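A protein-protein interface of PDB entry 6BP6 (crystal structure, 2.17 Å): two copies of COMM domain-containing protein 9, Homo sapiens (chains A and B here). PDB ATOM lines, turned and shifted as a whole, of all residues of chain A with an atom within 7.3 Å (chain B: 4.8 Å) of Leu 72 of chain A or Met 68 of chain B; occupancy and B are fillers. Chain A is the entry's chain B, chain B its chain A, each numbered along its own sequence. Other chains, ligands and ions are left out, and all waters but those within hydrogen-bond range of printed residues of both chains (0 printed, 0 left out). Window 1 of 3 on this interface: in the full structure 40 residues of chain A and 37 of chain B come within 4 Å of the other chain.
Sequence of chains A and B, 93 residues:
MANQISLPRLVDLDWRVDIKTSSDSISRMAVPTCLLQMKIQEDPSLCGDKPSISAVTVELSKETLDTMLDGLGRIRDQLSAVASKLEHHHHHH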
ATOM      1  N   LEU A  10      16.257  16.321  13.307  1.00  0.00           N
ATOM      2  CA  LEU A  10      16.916  15.200  12.651  1.00  0.00           C
ATOM      3  C   LEU A  10      16.360  15.070  11.238  1.00  0.00           C
ATOM      4  O   LEU A  10      15.163  14.821  11.067  1.00  0.00           O
ATOM      5  CB  LEU A  10      16.700  13.917  13.449  1.00  0.00           C
ATOM      6  CG  LEU A  10      17.237  12.638  12.810  1.00  0.00           C
ATOM      7  CD1 LEU A  10      18.748  12.722  12.623  1.00  0.00           C
ATOM      8  CD2 LEU A  10      16.857  11.428  13.646  1.00  0.00           C
ATOM      9  N   LEU A  13      19.214  10.025   8.235  1.00  0.00           N
ATOM     10  CA  LEU A  13      19.760   8.898   8.977  1.00  0.00           C
ATOM     11  C   LEU A  13      20.308   7.905   7.968  1.00  0.00           C
ATOM     12  O   LEU A  13      19.548   7.364   7.163  1.00  0.00           O
ATOM     13  CB  LEU A  13      18.692   8.240   9.855  1.00  0.00           C
ATOM     14  CG  LEU A  13      19.154   7.046  10.694  1.00  0.00           C
ATOM     15  CD1 LEU A  13      19.608   7.513  12.060  1.00  0.00           C
ATOM     16  CD2 LEU A  13      18.053   6.005  10.815  1.00  0.00           C
ATOM     17  N   TRP A  15      23.739   4.818   7.281  1.00  0.00           N
ATOM     18  CA  TRP A  15      24.582   3.886   8.024  1.00  0.00           C
ATOM     19  C   TRP A  15      25.368   3.007   7.058  1.00  0.00           C
ATOM     20  O   TRP A  15      25.082   2.936   5.861  1.00  0.00           O
ATOM     21  CB  TRP A  15      23.747   3.022   8.975  1.00  0.00           C
ATOM     22  CG  TRP A  15      22.851   2.053   8.269  1.00  0.00           C
ATOM     23  CD1 TRP A  15      23.179   0.807   7.825  1.00  0.00           C
ATOM     24  CD2 TRP A  15      21.478   2.253   7.923  1.00  0.00           C
ATOM     25  NE1 TRP A  15      22.095   0.214   7.221  1.00  0.00           N
ATOM     26  CE2 TRP A  15      21.036   1.081   7.273  1.00  0.00           C
ATOM     27  CE3 TRP A  15      20.574   3.304   8.110  1.00  0.00           C
ATOM     28  CZ2 TRP A  15      19.740   0.933   6.806  1.00  0.00           C
ATOM     29  CZ3 TRP A  15      19.286   3.155   7.645  1.00  0.00           C
ATOM     30  CH2 TRP A  15      18.879   1.978   6.998  1.00  0.00           C
ATOM     31  N   LEU A  36      26.939   4.820  12.040  1.00  0.00           N
ATOM     32  CA  LEU A  36      25.672   5.524  11.909  1.00  0.00           C
ATOM     33  C   LEU A  36      25.931   7.016  11.768  1.00  0.00           C
ATOM     34  O   LEU A  36      26.659   7.608  12.570  1.00  0.00           O
ATOM     35  CB  LEU A  36      24.774   5.261  13.117  1.00  0.00           C
ATOM     36  CG  LEU A  36      23.415   5.964  13.134  1.00  0.00           C
ATOM     37  CD1 LEU A  36      22.493   5.399  12.060  1.00  0.00           C
ATOM     38  CD2 LEU A  36      22.774   5.858  14.507  1.00  0.00           C
ATOM     39  N   MET A  38      23.895  10.608  11.508  1.00  0.00           N
ATOM     40  CA  MET A  38      22.684  11.402  11.614  1.00  0.00           C
ATOM     41  C   MET A  38      22.964  12.828  11.165  1.00  0.00           C
ATOM     42  O   MET A  38      23.949  13.432  11.570  1.00  0.00           O
ATOM     43  CB  MET A  38      22.170  11.386  13.047  1.00  0.00           C
ATOM     44  CG  MET A  38      21.734  10.011  13.507  1.00  0.00           C
ATOM     45  SD  MET A  38      21.485   9.933  15.437  1.00  0.00           S
ATOM     46  CE  MET A  38      23.341  10.197  15.998  1.00  0.00           C
ATOM     47  N   ASP A  66      20.176  -2.442  20.246  1.00  0.00           N
ATOM     48  CA  ASP A  66      18.984  -2.967  20.906  1.00  0.00           C
ATOM     49  C   ASP A  66      18.510  -2.033  22.013  1.00  0.00           C
ATOM     50  O   ASP A  66      17.303  -1.824  22.191  1.00  0.00           O
ATOM     51  CB  ASP A  66      19.264  -4.360  21.469  1.00  0.00           C
ATOM     52  CG  ASP A  66      19.260  -5.427  20.402  1.00  0.00           C
ATOM     53  OD1 ASP A  66      18.610  -5.211  19.363  1.00  0.00           O
ATOM     54  OD2 ASP A  66      19.902  -6.480  20.601  1.00  0.00           O
ATOM     55  N   THR A  67      19.446  -1.465  22.770  1.00  0.00           N
ATOM     56  CA  THR A  67      19.065  -0.532  23.821  1.00  0.00           C
ATOM     57  C   THR A  67      18.457   0.740  23.239  1.00  0.00           C
ATOM     58  O   THR A  67      17.471   1.261  23.778  1.00  0.00           O
ATOM     59  CB  THR A  67      20.271  -0.202  24.698  1.00  0.00           C
ATOM     60  OG1 THR A  67      21.037  -1.392  24.921  1.00  0.00           O
ATOM     61  CG2 THR A  67      19.810   0.332  26.045  1.00  0.00           C
ATOM     62  N   MET A  68      19.025   1.252  22.145  1.00  0.00           N
ATOM     63  CA  MET A  68      18.447   2.402  21.456  1.00  0.00           C
ATOM     64  C   MET A  68      17.009   2.085  21.062  1.00  0.00           C
ATOM     65  O   MET A  68      16.114   2.915  21.208  1.00  0.00           O
ATOM     66  CB  MET A  68      19.243   2.773  20.198  1.00  0.00           C
ATOM     67  CG  MET A  68      20.652   3.321  20.397  1.00  0.00           C
ATOM     68  SD  MET A  68      20.704   4.956  21.431  1.00  0.00           S
ATOM     69  CE  MET A  68      19.438   6.033  20.396  1.00  0.00           C
ATOM     70  N   LEU A  69      16.805   0.878  20.533  1.00  0.00           N
ATOM     71  CA  LEU A  69      15.477   0.500  20.062  1.00  0.00           C
ATOM     72  C   LEU A  69      14.480   0.430  21.214  1.00  0.00           C
ATOM     73  O   LEU A  69      13.341   0.892  21.085  1.00  0.00           O
ATOM     74  CB  LEU A  69      15.549  -0.827  19.304  1.00  0.00           C
ATOM     75  CG  LEU A  69      16.185  -0.715  17.911  1.00  0.00           C
ATOM     76  CD1 LEU A  69      16.442  -2.081  17.293  1.00  0.00           C
ATOM     77  CD2 LEU A  69      15.308   0.126  16.999  1.00  0.00           C
ATOM     78  N   ASP A  70      14.893  -0.133  22.355  1.00  0.00           N
ATOM     79  CA  ASP A  70      14.030  -0.138  23.538  1.00  0.00           C
ATOM     80  C   ASP A  70      13.677   1.283  23.972  1.00  0.00           C
ATOM     81  O   ASP A  70      12.509   1.594  24.255  1.00  0.00           O
ATOM     82  CB  ASP A  70      14.706  -0.885  24.690  1.00  0.00           C
ATOM     83  CG  ASP A  70      14.627  -2.388  24.546  1.00  0.00           C
ATOM     84  OD1 ASP A  70      13.574  -2.889  24.099  1.00  0.00           O
ATOM     85  OD2 ASP A  70      15.619  -3.068  24.882  1.00  0.00           O
ATOM     86  N   GLY A  71      14.682   2.157  24.046  1.00  0.00           N
ATOM     87  CA  GLY A  71      14.425   3.528  24.459  1.00  0.00           C
ATOM     88  C   GLY A  71      13.458   4.238  23.530  1.00  0.00           C
ATOM     89  O   GLY A  71      12.508   4.890  23.975  1.00  0.00           O
ATOM     90  N   LEU A  72      13.683   4.113  22.223  1.00  0.00           N
ATOM     91  CA  LEU A  72      12.812   4.788  21.268  1.00  0.00           C
ATOM     92  C   LEU A  72      11.408   4.200  21.280  1.00  0.00           C
ATOM     93  O   LEU A  72      10.433   4.928  21.058  1.00  0.00           O
ATOM     94  CB  LEU A  72      13.419   4.724  19.869  1.00  0.00           C
ATOM     95  CG  LEU A  72      14.743   5.468  19.673  1.00  0.00           C
ATOM     96  CD1 LEU A  72      15.107   5.490  18.203  1.00  0.00           C
ATOM     97  CD2 LEU A  72      14.670   6.881  20.229  1.00  0.00           C
ATOM     98  N   GLY A  73      11.275   2.899  21.554  1.00  0.00           N
ATOM     99  CA  GLY A  73       9.950   2.330  21.738  1.00  0.00           C
ATOM    100  C   GLY A  73       9.228   2.902  22.943  1.00  0.00           C
ATOM    101  O   GLY A  73       8.027   3.185  22.883  1.00  0.00           O
ATOM    102  N   ARG A  74       9.947   3.077  24.058  1.00  0.00           N
ATOM    103  CA  ARG A  74       9.334   3.688  25.236  1.00  0.00           C
ATOM    104  C   ARG A  74       8.910   5.124  24.948  1.00  0.00           C
ATOM    105  O   ARG A  74       7.859   5.582  25.418  1.00  0.00           O
ATOM    106  CB  ARG A  74      10.299   3.646  26.421  1.00  0.00           C
ATOM    107  CG  ARG A  74      10.577   2.254  26.969  1.00  0.00           C
ATOM    108  CD  ARG A  74      11.909   2.226  27.706  1.00  0.00           C
ATOM    109  NE  ARG A  74      12.045   3.344  28.636  1.00  0.00           N
ATOM    110  CZ  ARG A  74      11.750   3.279  29.931  1.00  0.00           C
ATOM    111  NH1 ARG A  74      11.901   4.348  30.704  1.00  0.00           N
ATOM    112  NH2 ARG A  74      11.305   2.145  30.456  1.00  0.00           N
ATOM    113  N   ILE A  75       9.719   5.851  24.172  1.00  0.00           N
ATOM    114  CA  ILE A  75       9.344   7.208  23.776  1.00  0.00           C
ATOM    115  C   ILE A  75       8.075   7.186  22.934  1.00  0.00           C
ATOM    116  O   ILE A  75       7.182   8.024  23.107  1.00  0.00           O
ATOM    117  CB  ILE A  75      10.495   7.892  23.020  1.00  0.00           C
ATOM    118  CG1 ILE A  75      11.722   8.026  23.911  1.00  0.00           C
ATOM    119  CG2 ILE A  75      10.051   9.248  22.515  1.00  0.00           C
ATOM    120  CD1 ILE A  75      12.934   8.525  23.176  1.00  0.00           C
ATOM    121  N   ARG A  76       7.994   6.248  21.986  1.00  0.00           N
ATOM    122  CA  ARG A  76       6.788   6.113  21.174  1.00  0.00           C
ATOM    123  C   ARG A  76       5.564   5.862  22.042  1.00  0.00           C
ATOM    124  O   ARG A  76       4.502   6.466  21.830  1.00  0.00           O
ATOM    125  CB  ARG A  76       6.967   4.980  20.162  1.00  0.00           C
ATOM    126  CG  ARG A  76       5.732   4.655  19.344  1.00  0.00           C
ATOM    127  CD  ARG A  76       6.036   3.563  18.332  1.00  0.00           C
ATOM    128  NE  ARG A  76       4.850   3.125  17.602  1.00  0.00           N
ATOM    129  CZ  ARG A  76       4.872   2.241  16.609  1.00  0.00           C
ATOM    130  NH1 ARG A  76       6.024   1.701  16.225  1.00  0.00           N
ATOM    131  NH2 ARG A  76       3.745   1.897  15.999  1.00  0.00           N
ATOM    132  N   ASP A  77       5.697   4.976  23.030  1.00  0.00           N
ATOM    133  CA  ASP A  77       4.577   4.685  23.920  1.00  0.00           C
ATOM    134  C   ASP A  77       4.164   5.920  24.713  1.00  0.00           C
ATOM    135  O   ASP A  77       2.965   6.178  24.889  1.00  0.00           O
ATOM    136  CB  ASP A  77       4.935   3.537  24.860  1.00  0.00           C
ATOM    137  CG  ASP A  77       5.169   2.235  24.121  1.00  0.00           C
ATOM    138  OD1 ASP A  77       4.763   2.136  22.941  1.00  0.00           O
ATOM    139  OD2 ASP A  77       5.748   1.307  24.723  1.00  0.00           O
ATOM    140  N   GLN A  78       5.135   6.697  25.199  1.00  0.00           N
ATOM    141  CA  GLN A  78       4.780   7.882  25.974  1.00  0.00           C
ATOM    142  C   GLN A  78       4.113   8.937  25.094  1.00  0.00           C
ATOM    143  O   GLN A  78       3.150   9.592  25.519  1.00  0.00           O
ATOM    144  CB  GLN A  78       6.013   8.454  26.676  1.00  0.00           C
ATOM    145  CG  GLN A  78       6.706   7.473  27.619  1.00  0.00           C
ATOM    146  CD  GLN A  78       5.734   6.671  28.476  1.00  0.00           C
ATOM    147  OE1 GLN A  78       5.710   5.440  28.419  1.00  0.00           O
ATOM    148  NE2 GLN A  78       4.938   7.365  29.284  1.00  0.00           N
ATOM    149  N   LEU A  79       4.598   9.102  23.861  1.00  0.00           N
ATOM    150  CA  LEU A  79       3.965  10.043  22.942  1.00  0.00           C
ATOM    151  C   LEU A  79       2.532   9.632  22.639  1.00  0.00           C
ATOM    152  O   LEU A  79       1.632  10.480  22.597  1.00  0.00           O
ATOM    153  CB  LEU A  79       4.768  10.149  21.644  1.00  0.00           C
ATOM    154  CG  LEU A  79       6.121  10.860  21.670  1.00  0.00           C
ATOM    155  CD1 LEU A  79       6.863  10.594  20.370  1.00  0.00           C
ATOM    156  CD2 LEU A  79       5.955  12.360  21.899  1.00  0.00           C
ATOM    157  N   LEU B  13      20.994   7.892  26.363  1.00  0.00           N
ATOM    158  CA  LEU B  13      19.824   8.357  25.629  1.00  0.00           C
ATOM    159  C   LEU B  13      18.795   8.793  26.656  1.00  0.00           C
ATOM    160  O   LEU B  13      18.335   7.972  27.455  1.00  0.00           O
ATOM    161  CB  LEU B  13      19.260   7.257  24.734  1.00  0.00           C
ATOM    162  CG  LEU B  13      17.995   7.642  23.976  1.00  0.00           C
ATOM    163  CD1 LEU B  13      18.357   8.544  22.816  1.00  0.00           C
ATOM    164  CD2 LEU B  13      17.239   6.408  23.500  1.00  0.00           C
ATOM    165  N   LEU B  36      14.756  14.899  22.579  1.00  0.00           N
ATOM    166  CA  LEU B  36      15.652  13.753  22.630  1.00  0.00           C
ATOM    167  C   LEU B  36      17.082  14.233  22.807  1.00  0.00           C
ATOM    168  O   LEU B  36      17.546  15.101  22.064  1.00  0.00           O
ATOM    169  CB  LEU B  36      15.543  12.919  21.353  1.00  0.00           C
ATOM    170  CG  LEU B  36      16.241  11.564  21.435  1.00  0.00           C
ATOM    171  CD1 LEU B  36      15.657  10.780  22.590  1.00  0.00           C
ATOM    172  CD2 LEU B  36      16.096  10.800  20.134  1.00  0.00           C
ATOM    173  N   LEU B  60      11.719  15.674  18.131  1.00  0.00           N
ATOM    174  CA  LEU B  60      11.116  14.652  17.284  1.00  0.00           C
ATOM    175  C   LEU B  60       9.601  14.695  17.393  1.00  0.00           C
ATOM    176  O   LEU B  60       9.049  14.797  18.496  1.00  0.00           O
ATOM    177  CB  LEU B  60      11.603  13.248  17.657  1.00  0.00           C
ATOM    178  CG  LEU B  60      13.095  12.952  17.560  1.00  0.00           C
ATOM    179  CD1 LEU B  60      13.356  11.494  17.884  1.00  0.00           C
ATOM    180  CD2 LEU B  60      13.611  13.285  16.180  1.00  0.00           C
ATOM    181  N   THR B  64       8.598  11.240  12.745  1.00  0.00           N
ATOM    182  CA  THR B  64      10.050  11.139  12.675  1.00  0.00           C
ATOM    183  C   THR B  64      10.559  10.016  13.569  1.00  0.00           C
ATOM    184  O   THR B  64      11.467   9.271  13.182  1.00  0.00           O
ATOM    185  CB  THR B  64      10.683  12.479  13.054  1.00  0.00           C
ATOM    186  OG1 THR B  64      10.203  13.488  12.160  1.00  0.00           O
ATOM    187  CG2 THR B  64      12.201  12.410  12.956  1.00  0.00           C
ATOM    188  N   LEU B  65       9.973   9.862  14.757  1.00  0.00           N
ATOM    189  CA  LEU B  65      10.363   8.760  15.630  1.00  0.00           C
ATOM    190  C   LEU B  65      10.052   7.410  14.994  1.00  0.00           C
ATOM    191  O   LEU B  65      10.874   6.488  15.053  1.00  0.00           O
ATOM    192  CB  LEU B  65       9.664   8.884  16.982  1.00  0.00           C
ATOM    193  CG  LEU B  65       9.923   7.725  17.945  1.00  0.00           C
ATOM    194  CD1 LEU B  65      11.403   7.597  18.247  1.00  0.00           C
ATOM    195  CD2 LEU B  65       9.143   7.911  19.220  1.00  0.00           C
ATOM    196  N   ASP B  66       8.868   7.271  14.390  1.00  0.00           N
ATOM    197  CA  ASP B  66       8.522   6.018  13.721  1.00  0.00           C
ATOM    198  C   ASP B  66       9.519   5.685  12.614  1.00  0.00           C
ATOM    199  O   ASP B  66       9.967   4.536  12.487  1.00  0.00           O
ATOM    200  CB  ASP B  66       7.101   6.101  13.156  1.00  0.00           C
ATOM    201  CG  ASP B  66       6.038   6.053  14.236  1.00  0.00           C
ATOM    202  OD1 ASP B  66       6.332   5.542  15.335  1.00  0.00           O
ATOM    203  OD2 ASP B  66       4.904   6.516  13.981  1.00  0.00           O
ATOM    204  N   THR B  67       9.879   6.681  11.804  1.00  0.00           N
ATOM    205  CA  THR B  67      10.833   6.443  10.725  1.00  0.00           C
ATOM    206  C   THR B  67      12.209   6.064  11.272  1.00  0.00           C
ATOM    207  O   THR B  67      12.877   5.168  10.732  1.00  0.00           O
ATOM    208  CB  THR B  67      10.921   7.678   9.828  1.00  0.00           C
ATOM    209  OG1 THR B  67       9.618   7.988   9.318  1.00  0.00           O
ATOM    210  CG2 THR B  67      11.859   7.421   8.662  1.00  0.00           C
ATOM    211  N   MET B  68      12.646   6.737  12.337  1.00  0.00           N
ATOM    212  CA  MET B  68      13.865   6.381  13.067  1.00  0.00           C
ATOM    213  C   MET B  68      13.864   4.918  13.479  1.00  0.00           C
ATOM    214  O   MET B  68      14.849   4.208  13.285  1.00  0.00           O
ATOM    215  CB  MET B  68      14.017   7.244  14.322  1.00  0.00           C
ATOM    216  CG  MET B  68      15.118   8.270  14.254  1.00  0.00           C
ATOM    217  SD  MET B  68      15.617   8.882  16.028  1.00  0.00           S
ATOM    218  CE  MET B  68      17.295   7.835  16.199  1.00  0.00           C
ATOM    219  N   LEU B  69      12.748   4.501  14.081  1.00  0.00           N
ATOM    220  CA  LEU B  69      12.610   3.122  14.537  1.00  0.00           C
ATOM    221  C   LEU B  69      12.722   2.145  13.376  1.00  0.00           C
ATOM    222  O   LEU B  69      13.388   1.109  13.490  1.00  0.00           O
ATOM    223  CB  LEU B  69      11.277   2.943  15.259  1.00  0.00           C
ATOM    224  CG  LEU B  69      11.240   3.408  16.715  1.00  0.00           C
ATOM    225  CD1 LEU B  69       9.806   3.547  17.200  1.00  0.00           C
ATOM    226  CD2 LEU B  69      12.005   2.430  17.586  1.00  0.00           C
ATOM    227  N   ASP B  70      12.075   2.457  12.254  1.00  0.00           N
ATOM    228  CA  ASP B  70      12.152   1.581  11.088  1.00  0.00           C
ATOM    229  C   ASP B  70      13.593   1.450  10.595  1.00  0.00           C
ATOM    230  O   ASP B  70      14.087   0.339  10.350  1.00  0.00           O
ATOM    231  CB  ASP B  70      11.236   2.111   9.982  1.00  0.00           C
ATOM    232  CG  ASP B  70      11.007   1.098   8.872  1.00  0.00           C
ATOM    233  OD1 ASP B  70      11.580  -0.012   8.942  1.00  0.00           O
ATOM    234  OD2 ASP B  70      10.251   1.410   7.926  1.00  0.00           O
ATOM    235  N   GLY B  71      14.294   2.581  10.475  1.00  0.00           N
ATOM    236  CA  GLY B  71      15.673   2.536  10.008  1.00  0.00           C
ATOM    237  C   GLY B  71      16.591   1.776  10.949  1.00  0.00           C
ATOM    238  O   GLY B  71      17.428   0.975  10.513  1.00  0.00           O
ATOM    239  N   LEU B  72      16.447   2.008  12.256  1.00  0.00           N
ATOM    240  CA  LEU B  72      17.306   1.307  13.200  1.00  0.00           C
ATOM    241  C   LEU B  72      16.987  -0.183  13.246  1.00  0.00           C
ATOM    242  O   LEU B  72      17.893  -0.997  13.452  1.00  0.00           O
ATOM    243  CB  LEU B  72      17.198   1.940  14.588  1.00  0.00           C
ATOM    244  CG  LEU B  72      17.779   3.353  14.772  1.00  0.00           C
ATOM    245  CD1 LEU B  72      17.591   3.829  16.200  1.00  0.00           C
ATOM    246  CD2 LEU B  72      19.248   3.416  14.392  1.00  0.00           C
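Of the 19 printed residues of chain A, 8 touch a printed residue of chain B.
Printed residues of chain A that touch a printed residue of chain B: Leu 10, Trp 15, Met 68, Leu 69, Leu 72, Ile 75, Arg 76 and Leu 79.
Hydrophobic or aromatic side chains of chain B that line the printed part of chain A: Leu 13, Leu 36, Leu 65, Met 68, Leu 69 and Leu 72.
Along chain B the printed residues that touch a printed residue of chain A span positions 13 to 72.
Among the printed residues, 14 pairs touch across the chains.
Of chain B, only Leu 65, Met 68, Leu 69 and Leu 72 come within 4 Å of Leu 72 of chain A.
Of chain A, only Leu 10 and Leu 72 come within 4 Å of Met 68 of chain B.
Of the printed residues of chain B, Arg 76 of chain A touches Leu 65, Asp 66 and Leu 69.
Printed residues of chain A within 4 Å of Leu 36 of chain B: Ile 75 (3.6 Å).
Of the printed residues of chain A, Gly 71 of chain B touches Trp 15 (3.9 Å).
Printed residues of chain B within 4 Å of Leu 10 of chain A: Met 68 (3.7 Å).
Arg 74 of chain A touches none of the printed residues of chain B.
Met 68 of chain A touches Leu 13 of chain B, but with the chains exchanged Leu 13 of chain A does not touch Met 68 of chain B (4.4 Å).
Leu 69 of chain A touches Leu 72 of chain B, and with the chains exchanged Leu 72 of chain A touches Leu 69 of chain B.
Leu 72 of chain A touches Met 68 of chain B, but with the chains exchanged Met 68 of chain A does not touch Leu 72 of chain B (4.5 Å).
Leu 72 of chain B touches its own counterpart, Leu 72 of chain A.
Positions printed for both chains: 13, 36, 66, 67, 68, 69, 70, 71 and 72.
The guanidinium group (NE) of Arg 76 of chain A is in salt-bridge range of the side-chain carboxylate (OD1) of Asp 66 of chain B (3.6 Å).
Among the printed residues, merely in contact across the chains: Leu 10 of chain A with Met 68 of chain B (3.7 Å), Trp 15 of chain A with Gly 71 of chain B (3.9 Å), Met 68 of chain A with Leu 13 of chain B (3.7 Å), Leu 69 of chain A with Leu 72 of chain B (3.6 Å), Leu 72 of chain A with Leu 65 of chain B (3.7 Å), Leu 72 of chain A with Met 68 of chain B (3.8 Å), Leu 72 of chain A with Leu 69 of chain B (3.5 Å), Leu 72 of chain A with Leu 72 of chain B (3.6 Å), Ile 75 of chain A with Leu 36 of chain B (3.6 Å), Ile 75 of chain A with Leu 65 of chain B (3.7 Å), Arg 76 of chain A with Leu 65 of chain B (3.4 Å), Arg 76 of chain A with Leu 69 of chain B (3.9 Å) and Leu 79 of chain A with Leu 65 of chain B (3.7 Å).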
